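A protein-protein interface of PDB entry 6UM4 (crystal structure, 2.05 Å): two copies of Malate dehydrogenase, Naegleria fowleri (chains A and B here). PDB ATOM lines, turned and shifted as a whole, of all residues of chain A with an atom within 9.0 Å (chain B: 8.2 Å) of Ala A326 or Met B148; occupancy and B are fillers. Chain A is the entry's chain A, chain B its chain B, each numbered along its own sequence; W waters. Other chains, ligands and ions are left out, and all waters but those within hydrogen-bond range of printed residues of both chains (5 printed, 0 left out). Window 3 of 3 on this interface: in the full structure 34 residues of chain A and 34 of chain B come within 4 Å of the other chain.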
ATOM      1  N   LEU A 251      -1.389 -11.932 -20.257  1.00  0.00           N
ATOM      2  CA  LEU A 251      -2.692 -12.449 -20.652  1.00  0.00           C
ATOM      3  C   LEU A 251      -3.581 -11.316 -21.162  1.00  0.00           C
ATOM      4  O   LEU A 251      -4.290 -11.477 -22.163  1.00  0.00           O
ATOM      5  CB  LEU A 251      -3.354 -13.203 -19.499  1.00  0.00           C
ATOM      6  CG  LEU A 251      -4.704 -13.789 -19.922  1.00  0.00           C
ATOM      7  CD1 LEU A 251      -4.535 -14.789 -21.067  1.00  0.00           C
ATOM      8  CD2 LEU A 251      -5.528 -14.372 -18.771  1.00  0.00           C
ATOM      9  N   ASP A 254      -2.204 -10.760 -24.651  1.00  0.00           N
ATOM     10  CA  ASP A 254      -2.659 -11.738 -25.623  1.00  0.00           C
ATOM     11  C   ASP A 254      -4.153 -11.609 -25.894  1.00  0.00           C
ATOM     12  O   ASP A 254      -4.615 -11.952 -26.991  1.00  0.00           O
ATOM     13  CB  ASP A 254      -2.317 -13.168 -25.147  1.00  0.00           C
ATOM     14  CG  ASP A 254      -0.816 -13.455 -25.183  1.00  0.00           C
ATOM     15  OD1 ASP A 254      -0.067 -12.711 -25.873  1.00  0.00           O
ATOM     16  OD2 ASP A 254      -0.378 -14.413 -24.499  1.00  0.00           O
ATOM     17  N   ARG A 255      -4.937 -11.195 -24.896  1.00  0.00           N
ATOM     18  CA  ARG A 255      -6.362 -11.004 -25.137  1.00  0.00           C
ATOM     19  C   ARG A 255      -6.598  -9.857 -26.106  1.00  0.00           C
ATOM     20  O   ARG A 255      -7.484  -9.940 -26.964  1.00  0.00           O
ATOM     21  CB  ARG A 255      -7.098 -10.763 -23.823  1.00  0.00           C
ATOM     22  CG  ARG A 255      -7.260 -12.018 -22.988  1.00  0.00           C
ATOM     23  CD  ARG A 255      -7.692 -11.672 -21.589  1.00  0.00           C
ATOM     24  NE  ARG A 255      -8.231 -12.830 -20.889  1.00  0.00           N
ATOM     25  CZ  ARG A 255      -8.463 -12.852 -19.586  1.00  0.00           C
ATOM     26  NH1 ARG A 255      -8.184 -11.782 -18.842  1.00  0.00           N
ATOM     27  NH2 ARG A 255      -8.955 -13.948 -19.025  1.00  0.00           N
ATOM     28  N   ALA A 258      -5.950 -11.059 -29.530  1.00  0.00           N
ATOM     29  CA  ALA A 258      -7.031 -11.872 -30.084  1.00  0.00           C
ATOM     30  C   ALA A 258      -8.210 -11.006 -30.490  1.00  0.00           C
ATOM     31  O   ALA A 258      -8.884 -11.315 -31.477  1.00  0.00           O
ATOM     32  CB  ALA A 258      -7.474 -12.965 -29.111  1.00  0.00           C
ATOM     33  N   GLN A 259      -8.479  -9.926 -29.750  1.00  0.00           N
ATOM     34  CA  GLN A 259      -9.566  -9.032 -30.158  1.00  0.00           C
ATOM     35  C   GLN A 259      -9.271  -8.403 -31.512  1.00  0.00           C
ATOM     36  O   GLN A 259     -10.144  -8.359 -32.385  1.00  0.00           O
ATOM     37  CB  GLN A 259      -9.811  -7.952 -29.098  1.00  0.00           C
ATOM     38  CG  GLN A 259     -10.438  -8.484 -27.791  1.00  0.00           C
ATOM     39  CD  GLN A 259     -11.833  -9.114 -28.006  1.00  0.00           C
ATOM     40  OE1 GLN A 259     -12.699  -8.532 -28.652  1.00  0.00           O
ATOM     41  NE2 GLN A 259     -12.035 -10.310 -27.463  1.00  0.00           N
ATOM     42  N   ASN A 315     -13.745  -4.691 -23.848  1.00  0.00           N
ATOM     43  CA  ASN A 315     -13.732  -6.132 -24.086  1.00  0.00           C
ATOM     44  C   ASN A 315     -12.467  -6.764 -23.524  1.00  0.00           C
ATOM     45  O   ASN A 315     -12.506  -7.878 -22.986  1.00  0.00           O
ATOM     46  CB  ASN A 315     -13.845  -6.440 -25.577  1.00  0.00           C
ATOM     47  CG  ASN A 315     -15.234  -6.187 -26.128  1.00  0.00           C
ATOM     48  OD1 ASN A 315     -16.213  -6.138 -25.384  1.00  0.00           O
ATOM     49  ND2 ASN A 315     -15.324  -6.032 -27.439  1.00  0.00           N
ATOM     50  N   GLN A 318     -12.689  -6.717 -19.608  1.00  0.00           N
ATOM     51  CA  GLN A 318     -13.729  -7.572 -19.046  1.00  0.00           C
ATOM     52  C   GLN A 318     -13.678  -8.992 -19.578  1.00  0.00           C
ATOM     53  O   GLN A 318     -14.626  -9.756 -19.376  1.00  0.00           O
ATOM     54  CB  GLN A 318     -15.110  -6.971 -19.311  1.00  0.00           C
ATOM     55  CG  GLN A 318     -15.235  -5.579 -18.749  1.00  0.00           C
ATOM     56  CD  GLN A 318     -15.012  -5.562 -17.249  1.00  0.00           C
ATOM     57  OE1 GLN A 318     -15.378  -6.509 -16.545  1.00  0.00           O
ATOM     58  NE2 GLN A 318     -14.383  -4.497 -16.756  1.00  0.00           N
ATOM     59  N   ARG A 319     -12.595  -9.356 -20.258  1.00  0.00           N
ATOM     60  CA  ARG A 319     -12.523 -10.658 -20.906  1.00  0.00           C
ATOM     61  C   ARG A 319     -12.633 -11.807 -19.903  1.00  0.00           C
ATOM     62  O   ARG A 319     -13.236 -12.846 -20.203  1.00  0.00           O
ATOM     63  CB  ARG A 319     -11.228 -10.747 -21.704  1.00  0.00           C
ATOM     64  CG  ARG A 319     -11.080 -12.068 -22.419  1.00  0.00           C
ATOM     65  CD  ARG A 319     -12.139 -12.284 -23.469  1.00  0.00           C
ATOM     66  NE  ARG A 319     -11.669 -13.288 -24.414  1.00  0.00           N
ATOM     67  CZ  ARG A 319     -12.229 -13.538 -25.592  1.00  0.00           C
ATOM     68  NH1 ARG A 319     -13.293 -12.860 -25.979  1.00  0.00           N
ATOM     69  NH2 ARG A 319     -11.711 -14.465 -26.379  1.00  0.00           N
ATOM     70  N   GLY A 320     -12.036 -11.658 -18.722  1.00  0.00           N
ATOM     71  CA  GLY A 320     -12.139 -12.717 -17.722  1.00  0.00           C
ATOM     72  C   GLY A 320     -13.571 -12.989 -17.306  1.00  0.00           C
ATOM     73  O   GLY A 320     -13.968 -14.141 -17.111  1.00  0.00           O
ATOM     74  N   ALA A 321     -14.363 -11.933 -17.139  1.00  0.00           N
ATOM     75  CA  ALA A 321     -15.753 -12.133 -16.757  1.00  0.00           C
ATOM     76  C   ALA A 321     -16.525 -12.838 -17.861  1.00  0.00           C
ATOM     77  O   ALA A 321     -17.436 -13.623 -17.574  1.00  0.00           O
ATOM     78  CB  ALA A 321     -16.403 -10.796 -16.405  1.00  0.00           C
ATOM     79  N   ALA A 322     -16.175 -12.576 -19.123  1.00  0.00           N
ATOM     80  CA  ALA A 322     -16.867 -13.224 -20.235  1.00  0.00           C
ATOM     81  C   ALA A 322     -16.618 -14.725 -20.248  1.00  0.00           C
ATOM     82  O   ALA A 322     -17.535 -15.511 -20.519  1.00  0.00           O
ATOM     83  CB  ALA A 322     -16.428 -12.607 -21.558  1.00  0.00           C
ATOM     84  N   ILE A 323     -15.377 -15.144 -19.996  1.00  0.00           N
ATOM     85  CA  ILE A 323     -15.073 -16.571 -19.970  1.00  0.00           C
ATOM     86  C   ILE A 323     -15.790 -17.262 -18.817  1.00  0.00           C
ATOM     87  O   ILE A 323     -16.297 -18.379 -18.970  1.00  0.00           O
ATOM     88  CB  ILE A 323     -13.551 -16.787 -19.941  1.00  0.00           C
ATOM     89  CG1 ILE A 323     -12.962 -16.330 -21.278  1.00  0.00           C
ATOM     90  CG2 ILE A 323     -13.217 -18.248 -19.658  1.00  0.00           C
ATOM     91  CD1 ILE A 323     -11.497 -16.363 -21.327  1.00  0.00           C
ATOM     92  N   ILE A 324     -15.841 -16.620 -17.647  1.00  0.00           N
ATOM     93  CA  ILE A 324     -16.559 -17.203 -16.512  1.00  0.00           C
ATOM     94  C   ILE A 324     -18.039 -17.368 -16.836  1.00  0.00           C
ATOM     95  O   ILE A 324     -18.663 -18.374 -16.466  1.00  0.00           O
ATOM     96  CB  ILE A 324     -16.344 -16.345 -15.252  1.00  0.00           C
ATOM     97  CG1 ILE A 324     -14.942 -16.567 -14.703  1.00  0.00           C
ATOM     98  CG2 ILE A 324     -17.387 -16.658 -14.184  1.00  0.00           C
ATOM     99  CD1 ILE A 324     -14.546 -15.550 -13.652  1.00  0.00           C
ATOM    100  N   LYS A 325     -18.625 -16.389 -17.532  1.00  0.00           N
ATOM    101  CA  LYS A 325     -20.039 -16.465 -17.880  1.00  0.00           C
ATOM    102  C   LYS A 325     -20.311 -17.607 -18.849  1.00  0.00           C
ATOM    103  O   LYS A 325     -21.358 -18.256 -18.773  1.00  0.00           O
ATOM    104  CB  LYS A 325     -20.498 -15.138 -18.478  1.00  0.00           C
ATOM    105  CG  LYS A 325     -21.962 -15.093 -18.868  1.00  0.00           C
ATOM    106  CD  LYS A 325     -22.318 -13.692 -19.409  1.00  0.00           C
ATOM    107  CE  LYS A 325     -23.746 -13.616 -19.934  1.00  0.00           C
ATOM    108  NZ  LYS A 325     -23.988 -12.366 -20.728  1.00  0.00           N
ATOM    109  N   ALA A 326     -19.381 -17.864 -19.768  1.00  0.00           N
ATOM    110  CA  ALA A 326     -19.569 -18.919 -20.761  1.00  0.00           C
ATOM    111  C   ALA A 326     -19.252 -20.314 -20.212  1.00  0.00           C
ATOM    112  O   ALA A 326     -19.992 -21.267 -20.482  1.00  0.00           O
ATOM    113  CB  ALA A 326     -18.712 -18.617 -21.987  1.00  0.00           C
ATOM    114  N   ARG A 327     -18.149 -20.468 -19.471  1.00  0.00           N
ATOM    115  CA  ARG A 327     -17.692 -21.784 -19.028  1.00  0.00           C
ATOM    116  C   ARG A 327     -18.109 -22.147 -17.610  1.00  0.00           C
ATOM    117  O   ARG A 327     -18.161 -23.340 -17.289  1.00  0.00           O
ATOM    118  CB  ARG A 327     -16.165 -21.872 -19.092  1.00  0.00           C
ATOM    119  CG  ARG A 327     -15.575 -21.645 -20.463  1.00  0.00           C
ATOM    120  CD  ARG A 327     -14.109 -22.051 -20.497  1.00  0.00           C
ATOM    121  NE  ARG A 327     -13.929 -23.497 -20.492  1.00  0.00           N
ATOM    122  CZ  ARG A 327     -12.803 -24.097 -20.850  1.00  0.00           C
ATOM    123  NH1 ARG A 327     -11.712 -23.370 -21.074  1.00  0.00           N
ATOM    124  NH2 ARG A 327     -12.727 -25.423 -20.846  1.00  0.00           N
ATOM    125  N   GLY A 328     -18.384 -21.170 -16.751  1.00  0.00           N
ATOM    126  CA  GLY A 328     -18.644 -21.453 -15.353  1.00  0.00           C
ATOM    127  C   GLY A 328     -17.403 -21.563 -14.494  1.00  0.00           C
ATOM    128  O   GLY A 328     -17.524 -21.792 -13.283  1.00  0.00           O
ATOM    129  N   LYS A 329     -16.219 -21.405 -15.078  1.00  0.00           N
ATOM    130  CA  LYS A 329     -14.961 -21.408 -14.351  1.00  0.00           C
ATOM    131  C   LYS A 329     -14.087 -20.324 -14.950  1.00  0.00           C
ATOM    132  O   LYS A 329     -14.332 -19.867 -16.068  1.00  0.00           O
ATOM    133  CB  LYS A 329     -14.248 -22.770 -14.428  1.00  0.00           C
ATOM    134  N   SER A 330     -13.065 -19.912 -14.202  1.00  0.00           N
ATOM    135  CA  SER A 330     -12.158 -18.885 -14.692  1.00  0.00           C
ATOM    136  C   SER A 330     -11.188 -19.480 -15.715  1.00  0.00           C
ATOM    137  O   SER A 330     -11.060 -20.700 -15.856  1.00  0.00           O
ATOM    138  CB  SER A 330     -11.390 -18.239 -13.540  1.00  0.00           C
ATOM    139  OG  SER A 330     -10.529 -19.196 -12.955  1.00  0.00           O
ATOM    140  N   SER A 331     -10.483 -18.593 -16.418  1.00  0.00           N
ATOM    141  CA  SER A 331      -9.685 -18.973 -17.586  1.00  0.00           C
ATOM    142  C   SER A 331      -8.283 -19.456 -17.193  1.00  0.00           C
ATOM    143  O   SER A 331      -7.266 -18.894 -17.592  1.00  0.00           O
ATOM    144  CB  SER A 331      -9.601 -17.791 -18.546  1.00  0.00           C
ATOM    145  OG  SER A 331      -9.292 -16.595 -17.848  1.00  0.00           O
ATOM    146  N   SER A 334      -5.686 -20.348 -20.234  1.00  0.00           N
ATOM    147  CA  SER A 334      -5.004 -19.241 -20.901  1.00  0.00           C
ATOM    148  C   SER A 334      -4.096 -18.458 -19.947  1.00  0.00           C
ATOM    149  O   SER A 334      -3.052 -17.958 -20.373  1.00  0.00           O
ATOM    150  CB  SER A 334      -6.016 -18.332 -21.633  1.00  0.00           C
ATOM    151  OG  SER A 334      -7.157 -18.035 -20.853  1.00  0.00           O
ATOM    152  N   CYS B 106     -15.242 -29.830 -24.625  1.00  0.00           N
ATOM    153  CA  CYS B 106     -15.433 -29.048 -23.406  1.00  0.00           C
ATOM    154  C   CYS B 106     -14.832 -29.685 -22.159  1.00  0.00           C
ATOM    155  O   CYS B 106     -14.798 -29.034 -21.108  1.00  0.00           O
ATOM    156  CB  CYS B 106     -16.917 -28.804 -23.150  1.00  0.00           C
ATOM    157  SG  CYS B 106     -17.460 -27.269 -23.873  1.00  0.00           S
ATOM    158  N   PHE B 115      -4.536 -26.735 -26.085  1.00  0.00           N
ATOM    159  CA  PHE B 115      -3.455 -25.753 -26.059  1.00  0.00           C
ATOM    160  C   PHE B 115      -2.146 -26.347 -26.548  1.00  0.00           C
ATOM    161  O   PHE B 115      -1.322 -25.630 -27.123  1.00  0.00           O
ATOM    162  CB  PHE B 115      -3.308 -25.204 -24.648  1.00  0.00           C
ATOM    163  CG  PHE B 115      -4.348 -24.198 -24.312  1.00  0.00           C
ATOM    164  CD1 PHE B 115      -4.046 -22.859 -24.299  1.00  0.00           C
ATOM    165  CD2 PHE B 115      -5.644 -24.594 -24.046  1.00  0.00           C
ATOM    166  CE1 PHE B 115      -5.024 -21.927 -24.032  1.00  0.00           C
ATOM    167  CE2 PHE B 115      -6.615 -23.661 -23.773  1.00  0.00           C
ATOM    168  CZ  PHE B 115      -6.299 -22.321 -23.760  1.00  0.00           C
ATOM    169  N   LEU B 133     -14.099 -28.437 -33.375  1.00  0.00           N
ATOM    170  CA  LEU B 133     -14.427 -28.820 -32.012  1.00  0.00           C
ATOM    171  C   LEU B 133     -15.876 -29.279 -31.955  1.00  0.00           C
ATOM    172  O   LEU B 133     -16.790 -28.530 -32.329  1.00  0.00           O
ATOM    173  CB  LEU B 133     -14.190 -27.675 -31.021  1.00  0.00           C
ATOM    174  CG  LEU B 133     -12.758 -27.140 -31.020  1.00  0.00           C
ATOM    175  CD1 LEU B 133     -12.541 -26.117 -29.904  1.00  0.00           C
ATOM    176  CD2 LEU B 133     -11.772 -28.287 -30.912  1.00  0.00           C
ATOM    177  N   ALA B 139     -23.868 -28.405 -24.472  1.00  0.00           N
ATOM    178  CA  ALA B 139     -22.586 -27.870 -24.045  1.00  0.00           C
ATOM    179  C   ALA B 139     -22.066 -26.802 -24.997  1.00  0.00           C
ATOM    180  O   ALA B 139     -20.921 -26.355 -24.857  1.00  0.00           O
ATOM    181  CB  ALA B 139     -21.568 -29.004 -23.915  1.00  0.00           C
ATOM    182  N   MET B 140     -22.892 -26.367 -25.947  1.00  0.00           N
ATOM    183  CA  MET B 140     -22.430 -25.431 -26.965  1.00  0.00           C
ATOM    184  C   MET B 140     -22.113 -24.062 -26.374  1.00  0.00           C
ATOM    185  O   MET B 140     -21.165 -23.405 -26.814  1.00  0.00           O
ATOM    186  CB  MET B 140     -23.470 -25.339 -28.078  1.00  0.00           C
ATOM    187  CG  MET B 140     -23.566 -26.642 -28.851  1.00  0.00           C
ATOM    188  SD  MET B 140     -21.933 -27.157 -29.429  1.00  0.00           S
ATOM    189  CE  MET B 140     -21.687 -25.903 -30.692  1.00  0.00           C
ATOM    190  N   LYS B 141     -22.881 -23.613 -25.374  1.00  0.00           N
ATOM    191  CA  LYS B 141     -22.561 -22.337 -24.735  1.00  0.00           C
ATOM    192  C   LYS B 141     -21.198 -22.393 -24.056  1.00  0.00           C
ATOM    193  O   LYS B 141     -20.406 -21.452 -24.160  1.00  0.00           O
ATOM    194  CB  LYS B 141     -23.645 -21.946 -23.730  1.00  0.00           C
ATOM    195  N   ALA B 142     -20.896 -23.502 -23.372  1.00  0.00           N
ATOM    196  CA  ALA B 142     -19.582 -23.652 -22.755  1.00  0.00           C
ATOM    197  C   ALA B 142     -18.473 -23.788 -23.793  1.00  0.00           C
ATOM    198  O   ALA B 142     -17.338 -23.367 -23.544  1.00  0.00           O
ATOM    199  CB  ALA B 142     -19.575 -24.857 -21.814  1.00  0.00           C
ATOM    200  N   LEU B 143     -18.754 -24.407 -24.934  1.00  0.00           N
ATOM    201  CA  LEU B 143     -17.713 -24.553 -25.945  1.00  0.00           C
ATOM    202  C   LEU B 143     -17.272 -23.210 -26.511  1.00  0.00           C
ATOM    203  O   LEU B 143     -16.118 -23.072 -26.937  1.00  0.00           O
ATOM    204  CB  LEU B 143     -18.197 -25.472 -27.062  1.00  0.00           C
ATOM    205  CG  LEU B 143     -17.155 -25.876 -28.108  1.00  0.00           C
ATOM    206  CD1 LEU B 143     -15.980 -26.609 -27.458  1.00  0.00           C
ATOM    207  CD2 LEU B 143     -17.795 -26.742 -29.200  1.00  0.00           C
ATOM    208  N   GLU B 144     -18.174 -22.227 -26.562  1.00  0.00           N
ATOM    209  CA  GLU B 144     -17.768 -20.878 -26.951  1.00  0.00           C
ATOM    210  C   GLU B 144     -16.690 -20.343 -26.020  1.00  0.00           C
ATOM    211  O   GLU B 144     -15.780 -19.630 -26.461  1.00  0.00           O
ATOM    212  CB  GLU B 144     -18.977 -19.950 -26.994  1.00  0.00           C
ATOM    213  CG  GLU B 144     -20.085 -20.466 -27.910  1.00  0.00           C
ATOM    214  CD  GLU B 144     -20.073 -19.850 -29.306  1.00  0.00           C
ATOM    215  OE1 GLU B 144     -18.983 -19.530 -29.823  1.00  0.00           O
ATOM    216  OE2 GLU B 144     -21.164 -19.726 -29.906  1.00  0.00           O
ATOM    217  N   GLY B 145     -16.784 -20.657 -24.724  1.00  0.00           N
ATOM    218  CA  GLY B 145     -15.718 -20.272 -23.809  1.00  0.00           C
ATOM    219  C   GLY B 145     -14.398 -20.944 -24.142  1.00  0.00           C
ATOM    220  O   GLY B 145     -13.333 -20.341 -24.002  1.00  0.00           O
ATOM    221  N   VAL B 146     -14.446 -22.214 -24.568  1.00  0.00           N
ATOM    222  CA  VAL B 146     -13.219 -22.902 -24.959  1.00  0.00           C
ATOM    223  C   VAL B 146     -12.549 -22.174 -26.117  1.00  0.00           C
ATOM    224  O   VAL B 146     -11.323 -22.018 -26.143  1.00  0.00           O
ATOM    225  CB  VAL B 146     -13.510 -24.377 -25.310  1.00  0.00           C
ATOM    226  CG1 VAL B 146     -12.267 -25.036 -25.854  1.00  0.00           C
ATOM    227  CG2 VAL B 146     -14.014 -25.139 -24.079  1.00  0.00           C
ATOM    228  N   LYS B 147     -13.333 -21.768 -27.118  1.00  0.00           N
ATOM    229  CA  LYS B 147     -12.789 -20.997 -28.237  1.00  0.00           C
ATOM    230  C   LYS B 147     -12.186 -19.678 -27.765  1.00  0.00           C
ATOM    231  O   LYS B 147     -11.142 -19.251 -28.267  1.00  0.00           O
ATOM    232  CB  LYS B 147     -13.878 -20.711 -29.273  1.00  0.00           C
ATOM    233  CG  LYS B 147     -13.424 -19.814 -30.425  1.00  0.00           C
ATOM    234  CD  LYS B 147     -14.563 -19.587 -31.401  1.00  0.00           C
ATOM    235  CE  LYS B 147     -14.181 -18.614 -32.504  1.00  0.00           C
ATOM    236  NZ  LYS B 147     -13.803 -17.302 -31.921  1.00  0.00           N
ATOM    237  N   MET B 148     -12.858 -19.002 -26.838  1.00  0.00           N
ATOM    238  CA  MET B 148     -12.355 -17.736 -26.315  1.00  0.00           C
ATOM    239  C   MET B 148     -10.966 -17.890 -25.685  1.00  0.00           C
ATOM    240  O   MET B 148     -10.055 -17.097 -25.968  1.00  0.00           O
ATOM    241  CB  MET B 148     -13.359 -17.189 -25.308  1.00  0.00           C
ATOM    242  CG  MET B 148     -14.564 -16.536 -25.936  1.00  0.00           C
ATOM    243  SD  MET B 148     -15.666 -15.931 -24.647  1.00  0.00           S
ATOM    244  CE  MET B 148     -16.964 -17.141 -24.702  1.00  0.00           C
ATOM    245  N   GLU B 149     -10.783 -18.921 -24.848  1.00  0.00           N
ATOM    246  CA  GLU B 149      -9.489 -19.164 -24.208  1.00  0.00           C
ATOM    247  C   GLU B 149      -8.424 -19.526 -25.228  1.00  0.00           C
ATOM    248  O   GLU B 149      -7.262 -19.145 -25.079  1.00  0.00           O
ATOM    249  CB  GLU B 149      -9.599 -20.266 -23.154  1.00  0.00           C
ATOM    250  CG  GLU B 149     -10.298 -19.837 -21.881  1.00  0.00           C
ATOM    251  CD  GLU B 149      -9.738 -20.524 -20.637  1.00  0.00           C
ATOM    252  OE1 GLU B 149     -10.433 -21.425 -20.117  1.00  0.00           O
ATOM    253  OE2 GLU B 149      -8.618 -20.161 -20.179  1.00  0.00           O
ATOM    254  N   LEU B 150      -8.785 -20.310 -26.238  1.00  0.00           N
ATOM    255  CA  LEU B 150      -7.815 -20.653 -27.275  1.00  0.00           C
ATOM    256  C   LEU B 150      -7.420 -19.425 -28.087  1.00  0.00           C
ATOM    257  O   LEU B 150      -6.230 -19.198 -28.354  1.00  0.00           O
ATOM    258  CB  LEU B 150      -8.397 -21.727 -28.196  1.00  0.00           C
ATOM    259  CG  LEU B 150      -8.384 -23.170 -27.691  1.00  0.00           C
ATOM    260  CD1 LEU B 150      -9.162 -24.082 -28.654  1.00  0.00           C
ATOM    261  CD2 LEU B 150      -6.980 -23.675 -27.459  1.00  0.00           C
ATOM    262  N   ASP B 151      -8.403 -18.608 -28.481  1.00  0.00           N
ATOM    263  CA  ASP B 151      -8.063 -17.347 -29.122  1.00  0.00           C
ATOM    264  C   ASP B 151      -7.141 -16.540 -28.222  1.00  0.00           C
ATOM    265  O   ASP B 151      -6.184 -15.924 -28.695  1.00  0.00           O
ATOM    266  CB  ASP B 151      -9.319 -16.531 -29.437  1.00  0.00           C
ATOM    267  CG  ASP B 151     -10.186 -17.158 -30.525  1.00  0.00           C
ATOM    268  OD1 ASP B 151      -9.673 -17.897 -31.405  1.00  0.00           O
ATOM    269  OD2 ASP B 151     -11.402 -16.891 -30.480  1.00  0.00           O
ATOM    270  N   ASP B 152      -7.436 -16.519 -26.926  1.00  0.00           N
ATOM    271  CA  ASP B 152      -6.626 -15.779 -25.965  1.00  0.00           C
ATOM    272  C   ASP B 152      -5.245 -16.363 -25.756  1.00  0.00           C
ATOM    273  O   ASP B 152      -4.448 -15.749 -25.054  1.00  0.00           O
ATOM    274  CB  ASP B 152      -7.355 -15.652 -24.634  1.00  0.00           C
ATOM    275  CG  ASP B 152      -8.591 -14.746 -24.751  1.00  0.00           C
ATOM    276  OD1 ASP B 152      -8.709 -14.026 -25.771  1.00  0.00           O
ATOM    277  OD2 ASP B 152      -9.422 -14.722 -23.818  1.00  0.00           O
ATOM    278  N   GLY B 153      -4.942 -17.524 -26.321  1.00  0.00           N
ATOM    279  CA  GLY B 153      -3.566 -17.982 -26.421  1.00  0.00           C
ATOM    280  C   GLY B 153      -2.748 -17.306 -27.499  1.00  0.00           C
ATOM    281  O   GLY B 153      -1.529 -17.469 -27.532  1.00  0.00           O
ATOM    282  N   ALA B 154      -3.396 -16.573 -28.403  1.00  0.00           N
ATOM    283  CA  ALA B 154      -2.711 -15.817 -29.450  1.00  0.00           C
ATOM    284  C   ALA B 154      -1.729 -16.701 -30.214  1.00  0.00           C
ATOM    285  O   ALA B 154      -0.588 -16.318 -30.478  1.00  0.00           O
ATOM    286  CB  ALA B 154      -2.004 -14.588 -28.865  1.00  0.00           C
ATOM    287  N   ILE B 161     -10.740 -21.932 -35.595  1.00  0.00           N
ATOM    288  CA  ILE B 161     -11.474 -22.703 -34.594  1.00  0.00           C
ATOM    289  C   ILE B 161     -12.941 -22.769 -35.009  1.00  0.00           C
ATOM    290  O   ILE B 161     -13.623 -21.735 -35.083  1.00  0.00           O
ATOM    291  CB  ILE B 161     -11.338 -22.108 -33.186  1.00  0.00           C
ATOM    292  CG1 ILE B 161      -9.858 -21.998 -32.797  1.00  0.00           C
ATOM    293  CG2 ILE B 161     -12.106 -22.957 -32.179  1.00  0.00           C
ATOM    294  CD1 ILE B 161      -9.621 -21.295 -31.496  1.00  0.00           C
ATOM    295  N   LEU B 163     -16.688 -24.566 -34.196  1.00  0.00           N
ATOM    296  CA  LEU B 163     -17.477 -25.191 -33.136  1.00  0.00           C
ATOM    297  C   LEU B 163     -18.749 -25.797 -33.726  1.00  0.00           C
ATOM    298  O   LEU B 163     -19.382 -25.189 -34.592  1.00  0.00           O
ATOM    299  CB  LEU B 163     -17.864 -24.176 -32.068  1.00  0.00           C
ATOM    300  CG  LEU B 163     -16.743 -23.278 -31.547  1.00  0.00           C
ATOM    301  CD1 LEU B 163     -17.292 -22.348 -30.498  1.00  0.00           C
ATOM    302  CD2 LEU B 163     -15.622 -24.143 -30.992  1.00  0.00           C
HETATM  303  O   HOH W   1      -8.439 -15.887 -21.357  1.00  0.00           O
HETATM  304  O   HOH W   2      -9.524 -11.404 -26.176  1.00  0.00           O
HETATM  305  O   HOH W   3     -12.008 -27.896 -22.767  1.00  0.00           O
HETATM  306  O   HOH W   4      -2.072 -16.043 -23.578  1.00  0.00           O
HETATM  307  O   HOH W   5     -12.452 -14.874 -29.100  1.00  0.00           O
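Of the 21 printed residues of chain A, 9 touch a printed residue of chain B. Printed residues of chain A that touch a printed residue of chain B: Asp A254, Arg A255, Ala A258, Arg A319, Ile A323, Ala A326, Arg A327, Ser A331 and Ser A334. Hydrophobic or aromatic side chains of chain A that line the printed part of chain B: Ala A258, Ile A323 and Ala A326. Of the 21 printed residues of chain B, 9 touch a printed residue of chain A. Hydrophobic or aromatic side chains of chain B within 4 Å of the printed part of chain A: Ala B142, Val B146, Met B148 and Ala B154. Among the printed residues, Asp or Glu carboxylates within 4 Å of a Lys or Arg side-chain nitrogen of the other chain: Arg A255 with Asp B152 (3.7 Å), Arg A319 with Asp B152 (2.7 Å) and Arg A327 with Glu B149 (2.5 Å).
No position is printed for both chains.
OD2 of Asp B152 is in salt-bridge range of NE of Arg A255, 3.7 Å away. OE1 of Glu B149 lies within salt-bridge range of NH1 of Arg A327 (2.5 Å). O of Met B148 is in hydrogen-bond range of NH2 of Arg A319, 3.1 Å away. The side-chain carboxylate of Glu B149 sits at hydrogen-bond distance from the side-chain hydroxyl of Ser A334. OE2 of Glu B149 sits close to O of Ser A331 (3.2 Å). NE of Arg A319 lies within salt-bridge range of OD2 of Asp B152 (2.7 Å).
Among the printed residues, pairs that only touch across the chains: Ala A258 with Asp B151, Ala A326 with Ala B142, Asp A254 with Asp B152, Arg A327 with Val B146, Ala A326 with Met B148, Arg A327 with Gly B145, Ile A323 with Asp B152, Ala A326 with Lys B141, Ala A258 with Asp B152, Ile A323 with Glu B149, Ala A326 with Gly B145, Arg A327 with Ala B142 and Asp A254 with Ala B154.
Of the printed residues of chain B, Asp A254 touches Asp B152 and Ala B154. Of chain B, only Lys B141, Ala B142, Gly B145 and Met B148 come within 4 Å of Ala A326. Of the printed residues of chain B, Ser A334 touches Glu B149. Of chain A, only Ala A326 and Arg A327 come within 4 Å of Gly B145. Met B148 touches just these residues of chain A: Arg A319 (3.1 Å) and Ala A326 (3.6 Å). Printed residues of chain A within 4 Å of Asp B152: Asp A254 (3.3 Å), Arg A255 (3.5 Å), Ala A258 (3.7 Å), Arg A319 (2.7 Å) and Ile A323 (3.6 Å). Of the printed residues of chain A, Ala B154 touches Asp A254 (3.99 Å). The nearest residue of chain B that does not touch Ala A326 is Glu B144 (4.8 Å).
Water W4 bridges the side-chain carboxylate (OD2) of Asp A254 (2.5 Å) and the backbone carbonyl oxygen (O) of Asp B152 (2.8 Å). Water W1 lies within hydrogen-bond range of the side-chain hydroxyl of Ser A334 (2.6 Å), the side-chain carboxylate of Asp B152 (2.9 Å) and the guanidinium group of Arg A255 (3.1 Å). Water W5 bridges OD2 of Asp B151 (2.7 Å) and NH2 of Arg A319 (2.8 Å).
OD2 of Asp B151 is in salt-bridge range of NZ of Lys B147 (2.8 Å). The guanidinium group (NH1) of Arg A319 lies close to the side-chain amide nitrogen (NE2) of Gln A259, at 3.2 Å. OG of Ser A334 lies close to O of Ser A331 (3.4 Å). The guanidinium group (NH2) of Arg A255 lies within hydrogen-bond range of the side-chain hydroxyl (OG) of Ser A331 (2.9 Å).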
